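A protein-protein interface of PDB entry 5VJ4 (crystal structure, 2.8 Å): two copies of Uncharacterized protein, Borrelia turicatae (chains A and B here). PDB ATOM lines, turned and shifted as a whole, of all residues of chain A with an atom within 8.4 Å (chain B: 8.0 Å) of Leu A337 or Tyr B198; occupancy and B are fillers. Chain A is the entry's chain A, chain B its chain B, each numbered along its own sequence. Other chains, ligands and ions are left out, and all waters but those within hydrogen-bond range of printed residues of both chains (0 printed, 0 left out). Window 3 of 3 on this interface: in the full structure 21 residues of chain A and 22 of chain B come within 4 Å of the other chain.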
ATOM      1  N   GLY A 328      -3.171  -1.994 -34.663  1.00  0.00           N
ATOM      2  CA  GLY A 328      -1.725  -2.259 -34.531  1.00  0.00           C
ATOM      3  C   GLY A 328      -1.285  -2.656 -33.119  1.00  0.00           C
ATOM      4  O   GLY A 328      -0.422  -3.519 -32.942  1.00  0.00           O
ATOM      5  N   THR A 329      -1.872  -2.030 -32.103  1.00  0.00           N
ATOM      6  CA  THR A 329      -1.400  -2.285 -30.769  1.00  0.00           C
ATOM      7  C   THR A 329      -1.903  -3.659 -30.315  1.00  0.00           C
ATOM      8  O   THR A 329      -1.186  -4.399 -29.641  1.00  0.00           O
ATOM      9  CB  THR A 329      -1.704  -1.117 -29.789  1.00  0.00           C
ATOM     10  OG1 THR A 329      -0.860  -1.221 -28.637  1.00  0.00           O
ATOM     11  CG2 THR A 329      -3.148  -1.108 -29.323  1.00  0.00           C
ATOM     12  N   PHE A 330      -3.108  -4.022 -30.714  1.00  0.00           N
ATOM     13  CA  PHE A 330      -3.608  -5.344 -30.346  1.00  0.00           C
ATOM     14  C   PHE A 330      -2.878  -6.471 -31.079  1.00  0.00           C
ATOM     15  O   PHE A 330      -2.501  -7.466 -30.466  1.00  0.00           O
ATOM     16  CB  PHE A 330      -5.098  -5.445 -30.589  1.00  0.00           C
ATOM     17  CG  PHE A 330      -5.895  -4.920 -29.473  1.00  0.00           C
ATOM     18  CD1 PHE A 330      -6.127  -5.701 -28.378  1.00  0.00           C
ATOM     19  CD2 PHE A 330      -6.380  -3.616 -29.487  1.00  0.00           C
ATOM     20  CE1 PHE A 330      -6.832  -5.219 -27.289  1.00  0.00           C
ATOM     21  CE2 PHE A 330      -7.106  -3.130 -28.424  1.00  0.00           C
ATOM     22  CZ  PHE A 330      -7.331  -3.947 -27.314  1.00  0.00           C
ATOM     23  N   LYS A 331      -2.678  -6.301 -32.385  1.00  0.00           N
ATOM     24  CA  LYS A 331      -1.978  -7.288 -33.174  1.00  0.00           C
ATOM     25  C   LYS A 331      -0.563  -7.496 -32.602  1.00  0.00           C
ATOM     26  O   LYS A 331      -0.168  -8.613 -32.245  1.00  0.00           O
ATOM     27  CB  LYS A 331      -1.951  -6.903 -34.663  1.00  0.00           C
ATOM     28  CG  LYS A 331      -0.868  -7.652 -35.441  1.00  0.00           C
ATOM     29  CD  LYS A 331      -0.972  -7.608 -36.959  1.00  0.00           C
ATOM     30  CE  LYS A 331      -0.255  -8.816 -37.555  1.00  0.00           C
ATOM     31  NZ  LYS A 331       0.376  -8.553 -38.879  1.00  0.00           N
ATOM     32  N   GLY A 332       0.181  -6.411 -32.490  1.00  0.00           N
ATOM     33  CA  GLY A 332       1.511  -6.479 -31.944  1.00  0.00           C
ATOM     34  C   GLY A 332       1.527  -7.131 -30.576  1.00  0.00           C
ATOM     35  O   GLY A 332       2.522  -7.749 -30.187  1.00  0.00           O
ATOM     36  N   PHE A 333       0.426  -7.017 -29.843  1.00  0.00           N
ATOM     37  CA  PHE A 333       0.409  -7.606 -28.528  1.00  0.00           C
ATOM     38  C   PHE A 333       0.342  -9.123 -28.661  1.00  0.00           C
ATOM     39  O   PHE A 333       1.212  -9.812 -28.157  1.00  0.00           O
ATOM     40  CB  PHE A 333      -0.754  -7.081 -27.732  1.00  0.00           C
ATOM     41  CG  PHE A 333      -0.689  -7.414 -26.282  1.00  0.00           C
ATOM     42  CD1 PHE A 333      -0.885  -8.717 -25.831  1.00  0.00           C
ATOM     43  CD2 PHE A 333      -0.459  -6.410 -25.347  1.00  0.00           C
ATOM     44  CE1 PHE A 333      -0.841  -9.018 -24.479  1.00  0.00           C
ATOM     45  CE2 PHE A 333      -0.402  -6.700 -23.989  1.00  0.00           C
ATOM     46  CZ  PHE A 333      -0.591  -8.008 -23.550  1.00  0.00           C
ATOM     47  N   THR A 334      -0.669  -9.639 -29.356  1.00  0.00           N
ATOM     48  CA  THR A 334      -0.773 -11.094 -29.528  1.00  0.00           C
ATOM     49  C   THR A 334       0.420 -11.658 -30.302  1.00  0.00           C
ATOM     50  O   THR A 334       0.766 -12.815 -30.124  1.00  0.00           O
ATOM     51  CB  THR A 334      -2.073 -11.523 -30.220  1.00  0.00           C
ATOM     52  OG1 THR A 334      -2.297 -10.626 -31.281  1.00  0.00           O
ATOM     53  CG2 THR A 334      -3.257 -11.450 -29.259  1.00  0.00           C
ATOM     54  N   ASP A 335       1.081 -10.835 -31.108  1.00  0.00           N
ATOM     55  CA  ASP A 335       2.262 -11.316 -31.836  1.00  0.00           C
ATOM     56  C   ASP A 335       3.546 -11.393 -31.032  1.00  0.00           C
ATOM     57  O   ASP A 335       4.549 -11.866 -31.550  1.00  0.00           O
ATOM     58  CB  ASP A 335       2.533 -10.505 -33.110  1.00  0.00           C
ATOM     59  CG  ASP A 335       1.500 -10.728 -34.180  1.00  0.00           C
ATOM     60  OD1 ASP A 335       1.480  -9.888 -35.093  1.00  0.00           O
ATOM     61  OD2 ASP A 335       0.721 -11.714 -34.124  1.00  0.00           O
ATOM     62  N   GLY A 336       3.545 -10.897 -29.803  1.00  0.00           N
ATOM     63  CA  GLY A 336       4.763 -10.943 -28.975  1.00  0.00           C
ATOM     64  C   GLY A 336       5.702  -9.758 -29.164  1.00  0.00           C
ATOM     65  O   GLY A 336       6.781  -9.709 -28.538  1.00  0.00           O
ATOM     66  N   LEU A 337       5.288  -8.792 -29.996  1.00  0.00           N
ATOM     67  CA  LEU A 337       6.093  -7.597 -30.291  1.00  0.00           C
ATOM     68  C   LEU A 337       6.237  -6.645 -29.107  1.00  0.00           C
ATOM     69  O   LEU A 337       7.300  -6.017 -28.949  1.00  0.00           O
ATOM     70  CB  LEU A 337       5.548  -6.857 -31.515  1.00  0.00           C
ATOM     71  CG  LEU A 337       6.045  -5.433 -31.809  1.00  0.00           C
ATOM     72  CD1 LEU A 337       7.562  -5.324 -32.000  1.00  0.00           C
ATOM     73  CD2 LEU A 337       5.296  -4.858 -33.005  1.00  0.00           C
ATOM     74  N   HIS A 338       5.161  -6.524 -28.320  1.00  0.00           N
ATOM     75  CA  HIS A 338       5.088  -5.625 -27.161  1.00  0.00           C
ATOM     76  C   HIS A 338       4.082  -6.095 -26.116  1.00  0.00           C
ATOM     77  O   HIS A 338       3.345  -7.071 -26.351  1.00  0.00           O
ATOM     78  CB  HIS A 338       4.800  -4.167 -27.587  1.00  0.00           C
ATOM     79  CG  HIS A 338       3.609  -3.995 -28.485  1.00  0.00           C
ATOM     80  ND1 HIS A 338       3.707  -3.449 -29.752  1.00  0.00           N
ATOM     81  CD2 HIS A 338       2.292  -4.250 -28.285  1.00  0.00           C
ATOM     82  CE1 HIS A 338       2.499  -3.380 -30.293  1.00  0.00           C
ATOM     83  NE2 HIS A 338       1.621  -3.848 -29.420  1.00  0.00           N
ATOM     84  N   PHE A 339       4.053  -5.402 -24.969  1.00  0.00           N
ATOM     85  CA  PHE A 339       3.281  -5.869 -23.820  1.00  0.00           C
ATOM     86  C   PHE A 339       2.407  -4.815 -23.179  1.00  0.00           C
ATOM     87  O   PHE A 339       2.019  -4.944 -22.008  1.00  0.00           O
ATOM     88  CB  PHE A 339       4.210  -6.551 -22.809  1.00  0.00           C
ATOM     89  CG  PHE A 339       5.047  -7.641 -23.421  1.00  0.00           C
ATOM     90  CD1 PHE A 339       6.283  -7.346 -24.012  1.00  0.00           C
ATOM     91  CD2 PHE A 339       4.580  -8.946 -23.470  1.00  0.00           C
ATOM     92  CE1 PHE A 339       7.045  -8.332 -24.599  1.00  0.00           C
ATOM     93  CE2 PHE A 339       5.341  -9.940 -24.066  1.00  0.00           C
ATOM     94  CZ  PHE A 339       6.576  -9.632 -24.627  1.00  0.00           C
ATOM     95  N   GLN A 340       2.057  -3.794 -23.965  1.00  0.00           N
ATOM     96  CA  GLN A 340       1.186  -2.699 -23.488  1.00  0.00           C
ATOM     97  C   GLN A 340       0.172  -2.350 -24.575  1.00  0.00           C
ATOM     98  O   GLN A 340       0.558  -2.216 -25.755  1.00  0.00           O
ATOM     99  CB  GLN A 340       1.995  -1.433 -23.210  1.00  0.00           C
ATOM    100  CG  GLN A 340       3.424  -1.569 -22.711  1.00  0.00           C
ATOM    101  CD  GLN A 340       3.534  -1.272 -21.242  1.00  0.00           C
ATOM    102  OE1 GLN A 340       2.614  -0.704 -20.644  1.00  0.00           O
ATOM    103  NE2 GLN A 340       4.656  -1.666 -20.643  1.00  0.00           N
ATOM    104  N   ILE B 127       6.993 -22.052 -28.641  1.00  0.00           N
ATOM    105  CA  ILE B 127       7.669 -20.749 -28.651  1.00  0.00           C
ATOM    106  C   ILE B 127       7.643 -20.053 -29.995  1.00  0.00           C
ATOM    107  O   ILE B 127       7.926 -18.880 -30.071  1.00  0.00           O
ATOM    108  CB  ILE B 127       9.141 -20.788 -28.198  1.00  0.00           C
ATOM    109  CG1 ILE B 127      10.002 -21.552 -29.206  1.00  0.00           C
ATOM    110  CG2 ILE B 127       9.238 -21.309 -26.777  1.00  0.00           C
ATOM    111  CD1 ILE B 127      11.481 -21.269 -29.052  1.00  0.00           C
ATOM    112  N   GLN B 128       7.321 -20.776 -31.055  1.00  0.00           N
ATOM    113  CA  GLN B 128       7.135 -20.158 -32.359  1.00  0.00           C
ATOM    114  C   GLN B 128       6.120 -19.022 -32.255  1.00  0.00           C
ATOM    115  O   GLN B 128       6.244 -18.011 -32.958  1.00  0.00           O
ATOM    116  CB  GLN B 128       6.653 -21.197 -33.368  1.00  0.00           C
ATOM    117  CG  GLN B 128       6.935 -20.874 -34.821  1.00  0.00           C
ATOM    118  CD  GLN B 128       6.100 -21.723 -35.747  1.00  0.00           C
ATOM    119  OE1 GLN B 128       6.184 -22.953 -35.729  1.00  0.00           O
ATOM    120  NE2 GLN B 128       5.267 -21.072 -36.552  1.00  0.00           N
ATOM    121  N   GLY B 129       5.145 -19.192 -31.348  1.00  0.00           N
ATOM    122  CA  GLY B 129       3.989 -18.306 -31.204  1.00  0.00           C
ATOM    123  C   GLY B 129       3.323 -18.053 -32.542  1.00  0.00           C
ATOM    124  O   GLY B 129       3.088 -18.983 -33.307  1.00  0.00           O
ATOM    125  N   ASN B 130       3.062 -16.786 -32.834  1.00  0.00           N
ATOM    126  CA  ASN B 130       2.506 -16.396 -34.113  1.00  0.00           C
ATOM    127  C   ASN B 130       3.541 -15.921 -35.120  1.00  0.00           C
ATOM    128  O   ASN B 130       3.193 -15.321 -36.146  1.00  0.00           O
ATOM    129  CB  ASN B 130       1.376 -15.385 -33.905  1.00  0.00           C
ATOM    130  CG  ASN B 130       0.088 -16.058 -33.479  1.00  0.00           C
ATOM    131  OD1 ASN B 130      -0.241 -17.159 -33.938  1.00  0.00           O
ATOM    132  ND2 ASN B 130      -0.646 -15.410 -32.604  1.00  0.00           N
ATOM    133  N   LEU B 131       4.812 -16.199 -34.824  1.00  0.00           N
ATOM    134  CA  LEU B 131       5.887 -15.933 -35.775  1.00  0.00           C
ATOM    135  C   LEU B 131       5.791 -17.018 -36.877  1.00  0.00           C
ATOM    136  O   LEU B 131       5.402 -18.157 -36.594  1.00  0.00           O
ATOM    137  CB  LEU B 131       7.260 -15.841 -35.058  1.00  0.00           C
ATOM    138  N   VAL B 135      10.341 -17.707 -40.674  1.00  0.00           N
ATOM    139  CA  VAL B 135      11.259 -16.902 -39.853  1.00  0.00           C
ATOM    140  C   VAL B 135      11.905 -17.725 -38.733  1.00  0.00           C
ATOM    141  O   VAL B 135      13.081 -17.514 -38.422  1.00  0.00           O
ATOM    142  CB  VAL B 135      10.611 -15.596 -39.316  1.00  0.00           C
ATOM    143  CG1 VAL B 135       9.419 -15.885 -38.414  1.00  0.00           C
ATOM    144  CG2 VAL B 135      11.640 -14.722 -38.599  1.00  0.00           C
ATOM    145  N   ARG B 139      16.089 -18.002 -38.472  1.00  0.00           N
ATOM    146  CA  ARG B 139      16.965 -17.835 -37.320  1.00  0.00           C
ATOM    147  C   ARG B 139      17.784 -19.090 -37.067  1.00  0.00           C
ATOM    148  O   ARG B 139      19.009 -19.009 -36.923  1.00  0.00           O
ATOM    149  CB  ARG B 139      16.190 -17.427 -36.056  1.00  0.00           C
ATOM    150  CG  ARG B 139      17.072 -17.118 -34.846  1.00  0.00           C
ATOM    151  CD  ARG B 139      17.831 -15.811 -35.012  1.00  0.00           C
ATOM    152  NE  ARG B 139      18.819 -15.587 -33.962  1.00  0.00           N
ATOM    153  CZ  ARG B 139      19.758 -14.648 -34.022  1.00  0.00           C
ATOM    154  NH1 ARG B 139      19.843 -13.845 -35.087  1.00  0.00           N
ATOM    155  NH2 ARG B 139      20.626 -14.515 -33.023  1.00  0.00           N
ATOM    156  N   GLY B 191       2.055 -15.944 -22.733  1.00  0.00           N
ATOM    157  CA  GLY B 191       2.344 -14.774 -23.585  1.00  0.00           C
ATOM    158  C   GLY B 191       3.747 -14.226 -23.348  1.00  0.00           C
ATOM    159  O   GLY B 191       4.484 -13.885 -24.293  1.00  0.00           O
ATOM    160  N   LEU B 192       4.132 -14.173 -22.079  1.00  0.00           N
ATOM    161  CA  LEU B 192       5.431 -13.646 -21.736  1.00  0.00           C
ATOM    162  C   LEU B 192       6.561 -14.478 -22.337  1.00  0.00           C
ATOM    163  O   LEU B 192       7.517 -13.927 -22.907  1.00  0.00           O
ATOM    164  CB  LEU B 192       5.560 -13.558 -20.224  1.00  0.00           C
ATOM    165  CG  LEU B 192       4.757 -12.407 -19.608  1.00  0.00           C
ATOM    166  CD1 LEU B 192       4.886 -12.471 -18.109  1.00  0.00           C
ATOM    167  CD2 LEU B 192       5.206 -11.042 -20.095  1.00  0.00           C
ATOM    168  N   VAL B 193       6.428 -15.803 -22.221  1.00  0.00           N
ATOM    169  CA  VAL B 193       7.432 -16.738 -22.708  1.00  0.00           C
ATOM    170  C   VAL B 193       7.513 -16.623 -24.216  1.00  0.00           C
ATOM    171  O   VAL B 193       8.604 -16.410 -24.765  1.00  0.00           O
ATOM    172  CB  VAL B 193       7.108 -18.187 -22.286  1.00  0.00           C
ATOM    173  CG1 VAL B 193       8.057 -19.183 -22.951  1.00  0.00           C
ATOM    174  CG2 VAL B 193       7.165 -18.334 -20.768  1.00  0.00           C
ATOM    175  N   LYS B 194       6.358 -16.714 -24.875  1.00  0.00           N
ATOM    176  CA  LYS B 194       6.295 -16.528 -26.320  1.00  0.00           C
ATOM    177  C   LYS B 194       6.947 -15.211 -26.748  1.00  0.00           C
ATOM    178  O   LYS B 194       7.521 -15.125 -27.833  1.00  0.00           O
ATOM    179  CB  LYS B 194       4.858 -16.613 -26.823  1.00  0.00           C
ATOM    180  CG  LYS B 194       4.213 -17.947 -26.502  1.00  0.00           C
ATOM    181  CD  LYS B 194       2.847 -18.073 -27.141  1.00  0.00           C
ATOM    182  CE  LYS B 194       2.257 -19.450 -26.898  1.00  0.00           C
ATOM    183  NZ  LYS B 194       1.019 -19.579 -27.718  1.00  0.00           N
ATOM    184  N   GLY B 195       6.863 -14.198 -25.892  1.00  0.00           N
ATOM    185  CA  GLY B 195       7.545 -12.932 -26.131  1.00  0.00           C
ATOM    186  C   GLY B 195       9.060 -13.029 -26.069  1.00  0.00           C
ATOM    187  O   GLY B 195       9.759 -12.508 -26.955  1.00  0.00           O
ATOM    188  N   ILE B 196       9.576 -13.702 -25.038  1.00  0.00           N
ATOM    189  CA  ILE B 196      11.019 -14.015 -24.968  1.00  0.00           C
ATOM    190  C   ILE B 196      11.450 -14.743 -26.241  1.00  0.00           C
ATOM    191  O   ILE B 196      12.505 -14.419 -26.819  1.00  0.00           O
ATOM    192  CB  ILE B 196      11.363 -14.876 -23.747  1.00  0.00           C
ATOM    193  CG1 ILE B 196      11.036 -14.120 -22.463  1.00  0.00           C
ATOM    194  CG2 ILE B 196      12.832 -15.262 -23.759  1.00  0.00           C
ATOM    195  CD1 ILE B 196      10.944 -15.006 -21.238  1.00  0.00           C
ATOM    196  N   GLY B 197      10.618 -15.704 -26.668  1.00  0.00           N
ATOM    197  CA  GLY B 197      10.750 -16.341 -27.978  1.00  0.00           C
ATOM    198  C   GLY B 197      10.897 -15.323 -29.098  1.00  0.00           C
ATOM    199  O   GLY B 197      11.974 -15.192 -29.683  1.00  0.00           O
ATOM    200  N   TYR B 198       9.812 -14.608 -29.393  1.00  0.00           N
ATOM    201  CA  TYR B 198       9.821 -13.512 -30.356  1.00  0.00           C
ATOM    202  C   TYR B 198      11.146 -12.751 -30.324  1.00  0.00           C
ATOM    203  O   TYR B 198      11.796 -12.568 -31.372  1.00  0.00           O
ATOM    204  CB  TYR B 198       8.688 -12.544 -30.044  1.00  0.00           C
ATOM    205  CG  TYR B 198       8.537 -11.433 -31.058  1.00  0.00           C
ATOM    206  CD1 TYR B 198       9.394 -10.303 -31.055  1.00  0.00           C
ATOM    207  CD2 TYR B 198       7.523 -11.499 -32.028  1.00  0.00           C
ATOM    208  CE1 TYR B 198       9.244  -9.291 -32.005  1.00  0.00           C
ATOM    209  CE2 TYR B 198       7.342 -10.488 -32.963  1.00  0.00           C
ATOM    210  CZ  TYR B 198       8.202  -9.396 -32.954  1.00  0.00           C
ATOM    211  OH  TYR B 198       7.993  -8.429 -33.895  1.00  0.00           O
ATOM    212  N   ASP B 199      11.537 -12.316 -29.124  1.00  0.00           N
ATOM    213  CA  ASP B 199      12.744 -11.508 -28.955  1.00  0.00           C
ATOM    214  C   ASP B 199      13.994 -12.228 -29.453  1.00  0.00           C
ATOM    215  O   ASP B 199      14.857 -11.624 -30.097  1.00  0.00           O
ATOM    216  CB  ASP B 199      12.914 -11.077 -27.493  1.00  0.00           C
ATOM    217  CG  ASP B 199      12.339  -9.696 -27.200  1.00  0.00           C
ATOM    218  OD1 ASP B 199      11.755  -9.030 -28.103  1.00  0.00           O
ATOM    219  OD2 ASP B 199      12.486  -9.292 -26.029  1.00  0.00           O
ATOM    220  N   PHE B 200      14.079 -13.522 -29.172  1.00  0.00           N
ATOM    221  CA  PHE B 200      15.202 -14.305 -29.637  1.00  0.00           C
ATOM    222  C   PHE B 200      15.177 -14.511 -31.155  1.00  0.00           C
ATOM    223  O   PHE B 200      16.213 -14.394 -31.808  1.00  0.00           O
ATOM    224  CB  PHE B 200      15.259 -15.649 -28.925  1.00  0.00           C
ATOM    225  CG  PHE B 200      16.247 -16.591 -29.532  1.00  0.00           C
ATOM    226  CD1 PHE B 200      17.616 -16.400 -29.323  1.00  0.00           C
ATOM    227  CD2 PHE B 200      15.827 -17.636 -30.351  1.00  0.00           C
ATOM    228  CE1 PHE B 200      18.545 -17.241 -29.905  1.00  0.00           C
ATOM    229  CE2 PHE B 200      16.749 -18.470 -30.944  1.00  0.00           C
ATOM    230  CZ  PHE B 200      18.109 -18.273 -30.719  1.00  0.00           C
ATOM    231  N   PHE B 201      14.002 -14.827 -31.693  1.00  0.00           N
ATOM    232  CA  PHE B 201      13.863 -15.069 -33.125  1.00  0.00           C
ATOM    233  C   PHE B 201      14.239 -13.869 -34.015  1.00  0.00           C
ATOM    234  O   PHE B 201      14.948 -14.038 -35.001  1.00  0.00           O
ATOM    235  CB  PHE B 201      12.472 -15.595 -33.487  1.00  0.00           C
ATOM    236  CG  PHE B 201      12.269 -17.062 -33.211  1.00  0.00           C
ATOM    237  CD1 PHE B 201      13.338 -17.969 -33.192  1.00  0.00           C
ATOM    238  CD2 PHE B 201      10.979 -17.552 -33.013  1.00  0.00           C
ATOM    239  CE1 PHE B 201      13.118 -19.317 -32.946  1.00  0.00           C
ATOM    240  CE2 PHE B 201      10.759 -18.902 -32.775  1.00  0.00           C
ATOM    241  CZ  PHE B 201      11.827 -19.784 -32.747  1.00  0.00           C
ATOM    242  N   HIS B 202      13.789 -12.667 -33.670  1.00  0.00           N
ATOM    243  CA  HIS B 202      14.123 -11.489 -34.479  1.00  0.00           C
ATOM    244  C   HIS B 202      15.500 -10.921 -34.160  1.00  0.00           C
ATOM    245  O   HIS B 202      15.903  -9.919 -34.746  1.00  0.00           O
ATOM    246  CB  HIS B 202      13.061 -10.413 -34.349  1.00  0.00           C
ATOM    247  CG  HIS B 202      11.773 -10.774 -35.005  1.00  0.00           C
ATOM    248  ND1 HIS B 202      10.805 -11.526 -34.372  1.00  0.00           N
ATOM    249  CD2 HIS B 202      11.295 -10.499 -36.244  1.00  0.00           C
ATOM    250  CE1 HIS B 202       9.782 -11.702 -35.194  1.00  0.00           C
ATOM    251  NE2 HIS B 202      10.053 -11.086 -36.334  1.00  0.00           N
ATOM    252  N   GLY B 203      16.213 -11.560 -33.235  1.00  0.00           N
ATOM    253  CA  GLY B 203      17.632 -11.279 -33.010  1.00  0.00           C
ATOM    254  C   GLY B 203      17.945 -10.268 -31.935  1.00  0.00           C
ATOM    255  O   GLY B 203      19.099  -9.857 -31.775  1.00  0.00           O
ATOM    256  N   SER B 204      16.933  -9.868 -31.185  1.00  0.00           N
ATOM    257  CA  SER B 204      17.134  -8.874 -30.135  1.00  0.00           C
ATOM    258  C   SER B 204      17.912  -9.438 -28.952  1.00  0.00           C
ATOM    259  O   SER B 204      18.645  -8.699 -28.292  1.00  0.00           O
ATOM    260  CB  SER B 204      15.803  -8.285 -29.681  1.00  0.00           C
ATOM    261  OG  SER B 204      15.130  -7.736 -30.795  1.00  0.00           O
ATOM    262  N   ILE B 205      17.742 -10.732 -28.685  1.00  0.00           N
ATOM    263  CA  ILE B 205      18.586 -11.418 -27.707  1.00  0.00           C
ATOM    264  C   ILE B 205      19.285 -12.635 -28.300  1.00  0.00           C
ATOM    265  O   ILE B 205      18.770 -13.276 -29.224  1.00  0.00           O
ATOM    266  CB  ILE B 205      17.828 -11.818 -26.426  1.00  0.00           C
ATOM    267  CG1 ILE B 205      16.656 -12.746 -26.764  1.00  0.00           C
ATOM    268  CG2 ILE B 205      17.423 -10.567 -25.663  1.00  0.00           C
ATOM    269  CD1 ILE B 205      16.256 -13.665 -25.637  1.00  0.00           C
ATOM    270  N   PHE B 210      18.319 -16.154 -24.036  1.00  0.00           N
ATOM    271  CA  PHE B 210      17.096 -16.928 -24.182  1.00  0.00           C
ATOM    272  C   PHE B 210      17.061 -18.048 -23.157  1.00  0.00           C
ATOM    273  O   PHE B 210      16.123 -18.135 -22.394  1.00  0.00           O
ATOM    274  CB  PHE B 210      16.909 -17.516 -25.571  1.00  0.00           C
ATOM    275  CG  PHE B 210      15.695 -18.396 -25.672  1.00  0.00           C
ATOM    276  CD1 PHE B 210      15.693 -19.707 -25.170  1.00  0.00           C
ATOM    277  CD2 PHE B 210      14.542 -17.912 -26.240  1.00  0.00           C
ATOM    278  CE1 PHE B 210      14.555 -20.493 -25.254  1.00  0.00           C
ATOM    279  CE2 PHE B 210      13.399 -18.702 -26.334  1.00  0.00           C
ATOM    280  CZ  PHE B 210      13.407 -19.991 -25.839  1.00  0.00           C
ATOM    281  N   ARG B 280       7.596  -9.201 -15.575  1.00  0.00           N
ATOM    282  CA  ARG B 280       8.308  -8.715 -16.716  1.00  0.00           C
ATOM    283  C   ARG B 280       9.420  -7.786 -16.252  1.00  0.00           C
ATOM    284  O   ARG B 280      10.543  -7.839 -16.759  1.00  0.00           O
ATOM    285  CB  ARG B 280       7.358  -8.065 -17.718  1.00  0.00           C
ATOM    286  CG  ARG B 280       8.053  -7.785 -19.032  1.00  0.00           C
ATOM    287  CD  ARG B 280       7.038  -7.450 -20.090  1.00  0.00           C
ATOM    288  NE  ARG B 280       7.561  -6.420 -20.981  1.00  0.00           N
ATOM    289  CZ  ARG B 280       8.546  -6.596 -21.863  1.00  0.00           C
ATOM    290  NH1 ARG B 280       9.145  -7.775 -21.999  1.00  0.00           N
ATOM    291  NH2 ARG B 280       8.927  -5.576 -22.627  1.00  0.00           N
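The backbone carbonyl oxygen (O) of Phe A330 lies within hydrogen-bond range of the side-chain hydroxyl (OG1) of Thr A334.
The backbone carbonyl oxygen (O) of Lys A331 lies within hydrogen-bond range of the side-chain hydroxyl (OG1) of Thr A334 (3.1 Å).
The backbone carbonyl oxygen (O) of Gly A332 sits at hydrogen-bond distance from the backbone NH (N) of Leu A337.
ND1 of His B202 sits at hydrogen-bond distance from O of Tyr B198, at 3.3 Å.
Among the printed residues, pairs that only touch across the chains: Thr A334 with Asn B130 (3.9 Å), Asp A335 with Asn B130 (3.7 Å), Asp A335 with Tyr B198 (3.0 Å), Gly A336 with Tyr B198 (3.5 Å), Leu A337 with Tyr B198 (3.7 Å), Phe A339 with Gly B195 (3.8 Å) and Phe A339 with Arg B280 (3.2 Å).
Of the printed residues of chain B, Thr A334 touches Asn B130.
Gly A336 touches just one residue of chain B: Tyr B198 (3.5 Å).
Leu A337 touches just one residue of chain B: Tyr B198 (3.7 Å).
Of the printed residues of chain A, Asn B130 touches Thr A334 (3.9 Å) and Asp A335 (3.7 Å).
Of the printed residues of chain A, Gly B195 touches Phe A339 (3.8 Å).
Gly B197 touches none of the printed residues of chain A.
Tyr B198 touches just these residues of chain A: Asp A335, Gly A336 and Leu A337.
The nearest residue of chain B that does not touch Leu A337 is Asp B199 (5.4 Å).
The nearest printed residue of chain B that does not touch Thr A334 is Gly B129 (6.3 Å).
Hydrophobic or aromatic side chains of chain B that line the printed part of chain A: Tyr B198.
Printed residues of chain A that touch a printed residue of chain B: Thr A334, Asp A335, Gly A336, Leu A337 and Phe A339.
Hydrophobic or aromatic side chains of chain A within 4 Å of the printed part of chain B: Leu A337 and Phe A339.
Among the printed residues, no Asp or Glu carboxylate lies within 4 Å of a Lys or Arg side-chain nitrogen of the other chain.
No position is printed for both chains.
Of the 7 pairs that touch across the chains among the printed residues, none has its exchanged pair printed and touching as well.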
